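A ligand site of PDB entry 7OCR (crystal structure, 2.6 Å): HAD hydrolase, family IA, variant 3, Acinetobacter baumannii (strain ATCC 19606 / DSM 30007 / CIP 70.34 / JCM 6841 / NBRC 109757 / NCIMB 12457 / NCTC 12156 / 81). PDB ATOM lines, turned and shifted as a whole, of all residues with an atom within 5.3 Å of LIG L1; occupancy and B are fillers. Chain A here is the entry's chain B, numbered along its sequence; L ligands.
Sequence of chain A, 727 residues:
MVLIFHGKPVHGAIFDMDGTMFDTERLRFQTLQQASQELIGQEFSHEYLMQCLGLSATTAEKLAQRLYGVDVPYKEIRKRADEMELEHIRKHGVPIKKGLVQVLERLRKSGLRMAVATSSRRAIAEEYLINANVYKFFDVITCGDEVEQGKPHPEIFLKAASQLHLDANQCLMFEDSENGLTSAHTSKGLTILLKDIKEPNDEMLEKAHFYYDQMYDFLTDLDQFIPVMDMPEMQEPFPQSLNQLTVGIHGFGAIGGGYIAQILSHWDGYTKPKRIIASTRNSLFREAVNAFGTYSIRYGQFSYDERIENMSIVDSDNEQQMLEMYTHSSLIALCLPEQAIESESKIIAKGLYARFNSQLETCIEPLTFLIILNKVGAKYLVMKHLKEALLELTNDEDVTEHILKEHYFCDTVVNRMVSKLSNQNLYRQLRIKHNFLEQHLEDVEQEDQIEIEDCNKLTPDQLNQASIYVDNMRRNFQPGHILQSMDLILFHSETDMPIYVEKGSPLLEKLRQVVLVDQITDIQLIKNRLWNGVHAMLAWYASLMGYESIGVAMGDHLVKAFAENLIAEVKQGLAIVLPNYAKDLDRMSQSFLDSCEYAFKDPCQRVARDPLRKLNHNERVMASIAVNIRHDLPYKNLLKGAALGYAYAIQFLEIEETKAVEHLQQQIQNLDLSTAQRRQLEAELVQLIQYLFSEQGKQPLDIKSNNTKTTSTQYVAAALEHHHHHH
NH2 of Arg 609 lies within salt-bridge range of O8 of LIG L1, at 2.7 Å.
An oxygen (O3) of LIG L1 sits at hydrogen-bond distance from the guanidinium group of Arg 606 (2.7 Å).
An oxygen (O5) of LIG L1 is in hydrogen-bond range of a ring nitrogen (ND1) of His 535.
An oxygen (O2) of LIG L1 is in hydrogen-bond range of the side-chain amide nitrogen of Asn 532 (2.9 Å).
The side-chain amino group (NZ) of Lys 527 lies within hydrogen-bond range of an oxygen (O2) of LIG L1.
An oxygen (O9) of LIG L1 lies within salt-bridge range of the side-chain amino group (NZ) of Lys 614, at 3.0 Å.
O7 of LIG L1 is in salt-bridge range of NH2 of Arg 613 (3.0 Å).
An oxygen (O2) of LIG L1 is in hydrogen-bond range of the side-chain amide nitrogen (ND2) of Asn 374 (3.0 Å).
The guanidinium group (NH1) of Arg 620 is in salt-bridge range of an oxygen (O7) of LIG L1 (3.1 Å).
O1 of LIG L1 lies within hydrogen-bond range of O of Asn 415 (3.3 Å).
The guanidinium group (NH2) of Arg 609 lies within salt-bridge range of an oxygen (O9) of LG2 L2 (3.1 Å).
The guanidinium group (NH2) of Arg 606 sits at hydrogen-bond distance from an oxygen (O14) of LG2 L2 (2.9 Å).
The side-chain amide nitrogen (ND2) of Asn 374 lies within hydrogen-bond range of an oxygen (O13) of LG2 L2 (3.0 Å).
The backbone NH of Val 418 is in hydrogen-bond range of an oxygen (O14) of LG2 L2, at 3.3 Å.
A nitrogen (N7) of LG2 L2 is in hydrogen-bond range of the backbone carbonyl oxygen of Val 418.
An oxygen (O8) of LIG L1 is in hydrogen-bond range of an oxygen (O13) of LG2 L2 (2.6 Å).
Arg 416 touches LIG L1.
Met 417 touches LIG L1 (CG to C1, 3.7 Å).
CE3 of Trp 531 touches O1 of LIG L1 (3.4 Å).
Val 607 touches LIG L1 (CG1 to O5, 3.9 Å).
Hydrophobic or aromatic side chains within 4 Å of LIG L1: Met 417, Trp 531, His 535 and Val 607.
14 residues have an atom within 4 Å of LIG L1: Asn 374, Asn 415, Arg 416, Met 417, Lys 527, Trp 531, Asn 532, His 535, Arg 606, Val 607, Arg 609, Arg 613, Lys 614 and Arg 620.
The guanidinium group (NE) of Arg 609 sits at hydrogen-bond distance from the backbone carbonyl oxygen (O) of Arg 606, at 3.1 Å.
The backbone carbonyl oxygen of Arg 609 is in hydrogen-bond range of the side-chain amino group of Lys 614, at 3.0 Å.
NE of Arg 606 lies within hydrogen-bond range of O of Val 418 (3.1 Å).
OD1 of Asp 602 is in salt-bridge range of NE of Arg 606 (2.7 Å).
The backbone NH (N) of Asn 532 lies within hydrogen-bond range of the backbone carbonyl oxygen (O) of Lys 527, at 3.0 Å.
The backbone carbonyl oxygen of Val 414 lies within hydrogen-bond range of the side-chain amino group of Lys 527.
NZ of Lys 614 is in hydrogen-bond range of O of Val 607 (2.6 Å).
OD2 of Asp 610 is in salt-bridge range of NH1 of Arg 613 (3.2 Å).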
ATOM      1  N   ASN A 374      -8.009 -19.469   8.748  1.00  0.00           N
ATOM      2  CA  ASN A 374      -7.415 -20.124   9.937  1.00  0.00           C
ATOM      3  C   ASN A 374      -6.423 -21.191   9.469  1.00  0.00           C
ATOM      4  O   ASN A 374      -6.813 -22.368   9.377  1.00  0.00           O
ATOM      5  CB  ASN A 374      -8.484 -20.721  10.868  1.00  0.00           C
ATOM      6  CG  ASN A 374      -9.210 -19.677  11.697  1.00  0.00           C
ATOM      7  OD1 ASN A 374      -8.740 -18.545  11.842  1.00  0.00           O
ATOM      8  ND2 ASN A 374     -10.343 -20.044  12.258  1.00  0.00           N
ATOM      9  N   VAL A 414      -8.096 -13.018  13.030  1.00  0.00           N
ATOM     10  CA  VAL A 414      -9.502 -12.723  13.466  1.00  0.00           C
ATOM     11  C   VAL A 414      -9.810 -13.592  14.695  1.00  0.00           C
ATOM     12  O   VAL A 414      -9.823 -14.818  14.552  1.00  0.00           O
ATOM     13  CB  VAL A 414     -10.505 -12.986  12.328  1.00  0.00           C
ATOM     14  CG1 VAL A 414     -11.939 -12.802  12.779  1.00  0.00           C
ATOM     15  CG2 VAL A 414     -10.215 -12.115  11.108  1.00  0.00           C
ATOM     16  N   ASN A 415     -10.050 -12.950  15.845  1.00  0.00           N
ATOM     17  CA  ASN A 415     -10.323 -13.623  17.141  1.00  0.00           C
ATOM     18  C   ASN A 415     -11.836 -13.791  17.345  1.00  0.00           C
ATOM     19  O   ASN A 415     -12.220 -14.685  18.133  1.00  0.00           O
ATOM     20  CB  ASN A 415      -9.694 -12.875  18.324  1.00  0.00           C
ATOM     21  CG  ASN A 415      -8.176 -12.931  18.328  1.00  0.00           C
ATOM     22  OD1 ASN A 415      -7.574 -13.744  17.623  1.00  0.00           O
ATOM     23  ND2 ASN A 415      -7.552 -12.093  19.136  1.00  0.00           N
ATOM     24  N   ARG A 416     -12.654 -12.983  16.669  1.00  0.00           N
ATOM     25  CA  ARG A 416     -14.135 -12.973  16.830  1.00  0.00           C
ATOM     26  C   ARG A 416     -14.729 -14.296  16.317  1.00  0.00           C
ATOM     27  O   ARG A 416     -14.486 -14.648  15.149  1.00  0.00           O
ATOM     28  CB  ARG A 416     -14.764 -11.799  16.064  1.00  0.00           C
ATOM     29  CG  ARG A 416     -16.279 -11.739  16.171  1.00  0.00           C
ATOM     30  CD  ARG A 416     -16.916 -10.702  15.268  1.00  0.00           C
ATOM     31  NE  ARG A 416     -16.979  -9.396  15.896  1.00  0.00           N
ATOM     32  CZ  ARG A 416     -17.769  -8.393  15.509  1.00  0.00           C
ATOM     33  NH1 ARG A 416     -18.596  -8.543  14.487  1.00  0.00           N
ATOM     34  NH2 ARG A 416     -17.738  -7.245  16.157  1.00  0.00           N
ATOM     35  N   MET A 417     -15.493 -14.987  17.177  1.00  0.00           N
ATOM     36  CA  MET A 417     -16.312 -16.175  16.833  1.00  0.00           C
ATOM     37  C   MET A 417     -17.641 -15.704  16.230  1.00  0.00           C
ATOM     38  O   MET A 417     -18.318 -14.884  16.878  1.00  0.00           O
ATOM     39  CB  MET A 417     -16.609 -17.020  18.077  1.00  0.00           C
ATOM     40  CG  MET A 417     -15.373 -17.562  18.756  1.00  0.00           C
ATOM     41  SD  MET A 417     -15.705 -18.150  20.438  1.00  0.00           S
ATOM     42  CE  MET A 417     -14.052 -18.588  20.957  1.00  0.00           C
ATOM     43  N   VAL A 418     -17.995 -16.204  15.041  1.00  0.00           N
ATOM     44  CA  VAL A 418     -19.249 -15.833  14.323  1.00  0.00           C
ATOM     45  C   VAL A 418     -19.926 -17.106  13.792  1.00  0.00           C
ATOM     46  O   VAL A 418     -19.199 -18.014  13.324  1.00  0.00           O
ATOM     47  CB  VAL A 418     -18.992 -14.833  13.184  1.00  0.00           C
ATOM     48  CG1 VAL A 418     -20.279 -14.406  12.499  1.00  0.00           C
ATOM     49  CG2 VAL A 418     -18.211 -13.615  13.666  1.00  0.00           C
ATOM     50  N   LYS A 527      -2.623 -18.387  17.833  1.00  0.00           N
ATOM     51  CA  LYS A 527      -4.049 -18.397  17.432  1.00  0.00           C
ATOM     52  C   LYS A 527      -4.464 -19.817  17.023  1.00  0.00           C
ATOM     53  O   LYS A 527      -5.546 -20.256  17.460  1.00  0.00           O
ATOM     54  CB  LYS A 527      -4.262 -17.397  16.287  1.00  0.00           C
ATOM     55  CG  LYS A 527      -5.539 -17.564  15.471  1.00  0.00           C
ATOM     56  CD  LYS A 527      -6.800 -17.304  16.255  1.00  0.00           C
ATOM     57  CE  LYS A 527      -8.049 -17.387  15.388  1.00  0.00           C
ATOM     58  NZ  LYS A 527      -9.278 -17.157  16.175  1.00  0.00           N
ATOM     59  N   TRP A 531      -6.002 -21.229  20.657  1.00  0.00           N
ATOM     60  CA  TRP A 531      -7.441 -20.919  20.420  1.00  0.00           C
ATOM     61  C   TRP A 531      -8.092 -22.044  19.603  1.00  0.00           C
ATOM     62  O   TRP A 531      -8.805 -22.871  20.203  1.00  0.00           O
ATOM     63  CB  TRP A 531      -7.614 -19.552  19.745  1.00  0.00           C
ATOM     64  CG  TRP A 531      -7.421 -18.375  20.650  1.00  0.00           C
ATOM     65  CD1 TRP A 531      -6.341 -18.114  21.438  1.00  0.00           C
ATOM     66  CD2 TRP A 531      -8.332 -17.277  20.834  1.00  0.00           C
ATOM     67  NE1 TRP A 531      -6.519 -16.926  22.111  1.00  0.00           N
ATOM     68  CE2 TRP A 531      -7.734 -16.398  21.755  1.00  0.00           C
ATOM     69  CE3 TRP A 531      -9.591 -16.953  20.311  1.00  0.00           C
ATOM     70  CZ2 TRP A 531      -8.353 -15.215  22.174  1.00  0.00           C
ATOM     71  CZ3 TRP A 531     -10.205 -15.793  20.723  1.00  0.00           C
ATOM     72  CH2 TRP A 531      -9.587 -14.936  21.645  1.00  0.00           C
ATOM     73  N   ASN A 532      -7.844 -22.075  18.289  1.00  0.00           N
ATOM     74  CA  ASN A 532      -8.544 -22.941  17.300  1.00  0.00           C
ATOM     75  C   ASN A 532      -8.407 -24.416  17.693  1.00  0.00           C
ATOM     76  O   ASN A 532      -9.385 -25.165  17.510  1.00  0.00           O
ATOM     77  CB  ASN A 532      -8.021 -22.727  15.868  1.00  0.00           C
ATOM     78  CG  ASN A 532      -8.211 -21.311  15.366  1.00  0.00           C
ATOM     79  OD1 ASN A 532      -7.465 -20.850  14.500  1.00  0.00           O
ATOM     80  ND2 ASN A 532      -9.198 -20.609  15.882  1.00  0.00           N
ATOM     81  N   HIS A 535     -10.431 -25.125  20.916  1.00  0.00           N
ATOM     82  CA  HIS A 535     -11.837 -24.891  20.478  1.00  0.00           C
ATOM     83  C   HIS A 535     -12.379 -26.150  19.790  1.00  0.00           C
ATOM     84  O   HIS A 535     -13.519 -26.549  20.108  1.00  0.00           O
ATOM     85  CB  HIS A 535     -11.920 -23.657  19.570  1.00  0.00           C
ATOM     86  CG  HIS A 535     -13.249 -22.976  19.570  1.00  0.00           C
ATOM     87  ND1 HIS A 535     -13.756 -22.350  18.444  1.00  0.00           N
ATOM     88  CD2 HIS A 535     -14.177 -22.834  20.539  1.00  0.00           C
ATOM     89  CE1 HIS A 535     -14.939 -21.835  18.736  1.00  0.00           C
ATOM     90  NE2 HIS A 535     -15.221 -22.123  20.015  1.00  0.00           N
ATOM     91  N   ALA A 536     -11.590 -26.748  18.896  1.00  0.00           N
ATOM     92  CA  ALA A 536     -11.941 -27.951  18.106  1.00  0.00           C
ATOM     93  C   ALA A 536     -12.044 -29.170  19.023  1.00  0.00           C
ATOM     94  O   ALA A 536     -13.015 -29.935  18.879  1.00  0.00           O
ATOM     95  CB  ALA A 536     -10.928 -28.166  17.012  1.00  0.00           C
ATOM     96  N   ASP A 602     -23.401 -20.201  19.191  1.00  0.00           N
ATOM     97  CA  ASP A 602     -22.312 -20.853  18.426  1.00  0.00           C
ATOM     98  C   ASP A 602     -22.456 -22.371  18.532  1.00  0.00           C
ATOM     99  O   ASP A 602     -22.229 -22.938  19.608  1.00  0.00           O
ATOM    100  CB  ASP A 602     -20.932 -20.383  18.917  1.00  0.00           C
ATOM    101  CG  ASP A 602     -19.760 -20.812  18.043  1.00  0.00           C
ATOM    102  OD1 ASP A 602     -20.006 -21.245  16.892  1.00  0.00           O
ATOM    103  OD2 ASP A 602     -18.613 -20.710  18.517  1.00  0.00           O
ATOM    104  N   ARG A 606     -20.206 -26.472  13.760  1.00  0.00           N
ATOM    105  CA  ARG A 606     -19.370 -25.575  12.904  1.00  0.00           C
ATOM    106  C   ARG A 606     -17.948 -25.465  13.488  1.00  0.00           C
ATOM    107  O   ARG A 606     -17.026 -25.154  12.710  1.00  0.00           O
ATOM    108  CB  ARG A 606     -20.019 -24.197  12.745  1.00  0.00           C
ATOM    109  CG  ARG A 606     -19.770 -23.227  13.891  1.00  0.00           C
ATOM    110  CD  ARG A 606     -19.720 -21.781  13.449  1.00  0.00           C
ATOM    111  NE  ARG A 606     -19.022 -20.954  14.421  1.00  0.00           N
ATOM    112  CZ  ARG A 606     -17.699 -20.871  14.544  1.00  0.00           C
ATOM    113  NH1 ARG A 606     -16.902 -21.547  13.746  1.00  0.00           N
ATOM    114  NH2 ARG A 606     -17.177 -20.074  15.469  1.00  0.00           N
ATOM    115  N   VAL A 607     -17.779 -25.693  14.791  1.00  0.00           N
ATOM    116  CA  VAL A 607     -16.461 -25.639  15.495  1.00  0.00           C
ATOM    117  C   VAL A 607     -15.724 -26.960  15.266  1.00  0.00           C
ATOM    118  O   VAL A 607     -14.483 -26.940  15.247  1.00  0.00           O
ATOM    119  CB  VAL A 607     -16.635 -25.330  16.996  1.00  0.00           C
ATOM    120  CG1 VAL A 607     -15.304 -25.286  17.727  1.00  0.00           C
ATOM    121  CG2 VAL A 607     -17.400 -24.030  17.219  1.00  0.00           C
ATOM    122  N   ARG A 609     -16.191 -28.960  12.552  1.00  0.00           N
ATOM    123  CA  ARG A 609     -16.210 -29.257  11.089  1.00  0.00           C
ATOM    124  C   ARG A 609     -14.799 -29.602  10.609  1.00  0.00           C
ATOM    125  O   ARG A 609     -13.826 -29.043  11.170  1.00  0.00           O
ATOM    126  CB  ARG A 609     -16.787 -28.072  10.311  1.00  0.00           C
ATOM    127  CG  ARG A 609     -15.885 -26.848  10.265  1.00  0.00           C
ATOM    128  CD  ARG A 609     -16.589 -25.637   9.673  1.00  0.00           C
ATOM    129  NE  ARG A 609     -15.874 -24.401   9.937  1.00  0.00           N
ATOM    130  CZ  ARG A 609     -16.280 -23.186   9.564  1.00  0.00           C
ATOM    131  NH1 ARG A 609     -17.403 -23.042   8.888  1.00  0.00           N
ATOM    132  NH2 ARG A 609     -15.547 -22.131   9.861  1.00  0.00           N
ATOM    133  N   ASP A 610     -14.697 -30.487   9.617  1.00  0.00           N
ATOM    134  CA  ASP A 610     -13.443 -30.901   8.939  1.00  0.00           C
ATOM    135  C   ASP A 610     -12.448 -31.452   9.961  1.00  0.00           C
ATOM    136  O   ASP A 610     -11.335 -30.942  10.064  1.00  0.00           O
ATOM    137  CB  ASP A 610     -12.850 -29.729   8.144  1.00  0.00           C
ATOM    138  CG  ASP A 610     -13.857 -28.962   7.309  1.00  0.00           C
ATOM    139  OD1 ASP A 610     -14.868 -29.580   6.907  1.00  0.00           O
ATOM    140  OD2 ASP A 610     -13.632 -27.759   7.082  1.00  0.00           O
ATOM    141  N   ARG A 613      -8.801 -32.525   8.518  1.00  0.00           N
ATOM    142  CA  ARG A 613      -8.012 -31.310   8.170  1.00  0.00           C
ATOM    143  C   ARG A 613      -7.319 -30.773   9.437  1.00  0.00           C
ATOM    144  O   ARG A 613      -6.123 -30.461   9.352  1.00  0.00           O
ATOM    145  CB  ARG A 613      -8.907 -30.234   7.546  1.00  0.00           C
ATOM    146  CG  ARG A 613      -8.165 -29.026   7.006  1.00  0.00           C
ATOM    147  CD  ARG A 613      -9.097 -27.872   6.683  1.00  0.00           C
ATOM    148  NE  ARG A 613      -9.657 -27.268   7.882  1.00  0.00           N
ATOM    149  CZ  ARG A 613     -10.597 -26.326   7.894  1.00  0.00           C
ATOM    150  NH1 ARG A 613     -11.090 -25.859   6.765  1.00  0.00           N
ATOM    151  NH2 ARG A 613     -11.038 -25.848   9.045  1.00  0.00           N
ATOM    152  N   LYS A 614      -8.056 -30.694  10.546  1.00  0.00           N
ATOM    153  CA  LYS A 614      -7.571 -30.131  11.841  1.00  0.00           C
ATOM    154  C   LYS A 614      -6.654 -31.137  12.556  1.00  0.00           C
ATOM    155  O   LYS A 614      -5.953 -30.710  13.493  1.00  0.00           O
ATOM    156  CB  LYS A 614      -8.768 -29.745  12.718  1.00  0.00           C
ATOM    157  CG  LYS A 614      -9.622 -28.616  12.162  1.00  0.00           C
ATOM    158  CD  LYS A 614     -10.858 -28.301  12.982  1.00  0.00           C
ATOM    159  CE  LYS A 614     -11.658 -27.165  12.395  1.00  0.00           C
ATOM    160  NZ  LYS A 614     -12.950 -26.975  13.093  1.00  0.00           N
ATOM    161  N   ARG A 620      -3.585 -27.624  14.246  1.00  0.00           N
ATOM    162  CA  ARG A 620      -3.897 -27.130  15.618  1.00  0.00           C
ATOM    163  C   ARG A 620      -3.853 -28.244  16.683  1.00  0.00           C
ATOM    164  O   ARG A 620      -3.844 -27.883  17.875  1.00  0.00           O
ATOM    165  CB  ARG A 620      -5.275 -26.462  15.613  1.00  0.00           C
ATOM    166  CG  ARG A 620      -6.424 -27.370  15.205  1.00  0.00           C
ATOM    167  CD  ARG A 620      -7.588 -26.585  14.631  1.00  0.00           C
ATOM    168  NE  ARG A 620      -7.231 -25.937  13.373  1.00  0.00           N
ATOM    169  CZ  ARG A 620      -8.003 -25.079  12.706  1.00  0.00           C
ATOM    170  NH1 ARG A 620      -9.195 -24.750  13.176  1.00  0.00           N
ATOM    171  NH2 ARG A 620      -7.573 -24.558  11.573  1.00  0.00           N
HETATM  172  C1  LIG L   1     -12.423 -17.719  16.581  1.00  0.00           C
HETATM  173  C2  LIG L   1     -12.220 -18.863  15.644  1.00  0.00           C
HETATM  174  C3  LIG L   1     -13.206 -20.024  15.710  1.00  0.00           C
HETATM  175  C4  LIG L   1     -13.007 -21.047  14.587  1.00  0.00           C
HETATM  176  C5  LIG L   1     -13.506 -22.450  14.943  1.00  0.00           C
HETATM  177  C6  LIG L   1     -13.617 -23.374  13.748  1.00  0.00           C
HETATM  178  O1  LIG L   1     -11.763 -17.896  17.812  1.00  0.00           O
HETATM  179  O2  LIG L   1     -11.290 -18.875  14.866  1.00  0.00           O
HETATM  180  O3  LIG L   1     -14.531 -19.552  15.656  1.00  0.00           O
HETATM  181  O4  LIG L   1     -13.656 -20.584  13.399  1.00  0.00           O
HETATM  182  O5  LIG L   1     -12.627 -23.035  15.903  1.00  0.00           O
HETATM  183  O6  LIG L   1     -12.355 -23.389  13.018  1.00  0.00           O
HETATM  184  P1  LIG L   1     -12.390 -23.516  11.401  1.00  0.00           P
HETATM  185  O7  LIG L   1     -10.942 -23.564  10.948  1.00  0.00           O
HETATM  186  O8  LIG L   1     -13.115 -22.273  10.913  1.00  0.00           O
HETATM  187  O9  LIG L   1     -13.150 -24.785  11.101  1.00  0.00           O
HETATM  188  P1  LG2 L   2     -18.227 -20.318   5.935  1.00  0.00           P
HETATM  189  O1  LG2 L   2     -18.573 -21.737   5.634  1.00  0.00           O
HETATM  190  O2  LG2 L   2     -19.298 -19.341   6.361  1.00  0.00           O
HETATM  191  O3  LG2 L   2     -17.319 -19.731   4.679  1.00  0.00           O
HETATM  192  C1  LG2 L   2     -18.118 -18.756   4.067  1.00  0.00           C
HETATM  193  C2  LG2 L   2     -17.833 -18.666   2.579  1.00  0.00           C
HETATM  194  O4  LG2 L   2     -17.065 -19.781   2.126  1.00  0.00           O
HETATM  195  C3  LG2 L   2     -19.216 -18.644   1.842  1.00  0.00           C
HETATM  196  O5  LG2 L   2     -19.213 -17.694   0.839  1.00  0.00           O
HETATM  197  C4  LG2 L   2     -19.242 -20.053   1.220  1.00  0.00           C
HETATM  198  O6  LG2 L   2     -19.920 -20.127   0.075  1.00  0.00           O
HETATM  199  C5  LG2 L   2     -17.715 -20.241   0.946  1.00  0.00           C
HETATM  200  N1  LG2 L   2     -17.367 -21.651   0.755  1.00  0.00           N
HETATM  201  C6  LG2 L   2     -17.405 -22.697   1.693  1.00  0.00           C
HETATM  202  N2  LG2 L   2     -17.023 -23.885   1.192  1.00  0.00           N
HETATM  203  C7  LG2 L   2     -16.733 -23.594  -0.157  1.00  0.00           C
HETATM  204  C8  LG2 L   2     -16.292 -24.414  -1.212  1.00  0.00           C
HETATM  205  N3  LG2 L   2     -16.068 -25.756  -1.006  1.00  0.00           N
HETATM  206  N4  LG2 L   2     -16.064 -23.898  -2.470  1.00  0.00           N
HETATM  207  C9  LG2 L   2     -16.311 -22.534  -2.594  1.00  0.00           C
HETATM  208  N5  LG2 L   2     -16.731 -21.638  -1.691  1.00  0.00           N
HETATM  209  C10 LG2 L   2     -16.947 -22.206  -0.440  1.00  0.00           C
HETATM  210  O7  LG2 L   2     -17.283 -20.532   7.261  1.00  0.00           O
HETATM  211  P2  LG2 L   2     -16.527 -19.175   7.664  1.00  0.00           P
HETATM  212  O8  LG2 L   2     -17.073 -17.992   6.967  1.00  0.00           O
HETATM  213  O9  LG2 L   2     -16.171 -19.152   9.137  1.00  0.00           O
HETATM  214  O10 LG2 L   2     -14.932 -19.326   6.951  1.00  0.00           O
HETATM  215  C11 LG2 L   2     -14.331 -18.088   6.977  1.00  0.00           C
HETATM  216  C12 LG2 L   2     -12.812 -18.259   7.119  1.00  0.00           C
HETATM  217  O11 LG2 L   2     -12.395 -17.458   8.231  1.00  0.00           O
HETATM  218  C13 LG2 L   2     -12.421 -19.737   7.456  1.00  0.00           C
HETATM  219  O12 LG2 L   2     -11.134 -19.961   6.993  1.00  0.00           O
HETATM  220  C14 LG2 L   2     -12.470 -19.715   8.979  1.00  0.00           C
HETATM  221  O13 LG2 L   2     -11.628 -20.637   9.577  1.00  0.00           O
HETATM  222  C15 LG2 L   2     -11.898 -18.293   9.254  1.00  0.00           C
HETATM  223  N6  LG2 L   2     -12.369 -17.756  10.552  1.00  0.00           N
HETATM  224  C16 LG2 L   2     -13.709 -17.840  10.917  1.00  0.00           C
HETATM  225  C17 LG2 L   2     -14.098 -17.463  12.168  1.00  0.00           C
HETATM  226  C18 LG2 L   2     -15.444 -17.819  12.624  1.00  0.00           C
HETATM  227  O14 LG2 L   2     -15.694 -18.216  13.771  1.00  0.00           O
HETATM  228  N7  LG2 L   2     -16.513 -17.687  11.749  1.00  0.00           N
HETATM  229  C19 LG2 L   2     -13.209 -16.639  13.029  1.00  0.00           C
HETATM  230  C20 LG2 L   2     -11.789 -16.803  12.656  1.00  0.00           C
HETATM  231  C21 LG2 L   2     -11.446 -17.127  11.413  1.00  0.00           C
HETATM  232  P3  LG2 L   2     -21.715 -20.362   0.342  1.00  0.00           P
HETATM  233  O15 LG2 L   2     -22.040 -20.753  -1.055  1.00  0.00           O
HETATM  234  O16 LG2 L   2     -21.787 -21.456   1.420  1.00  0.00           O
HETATM  235  O17 LG2 L   2     -22.043 -18.958   0.768  1.00  0.00           O
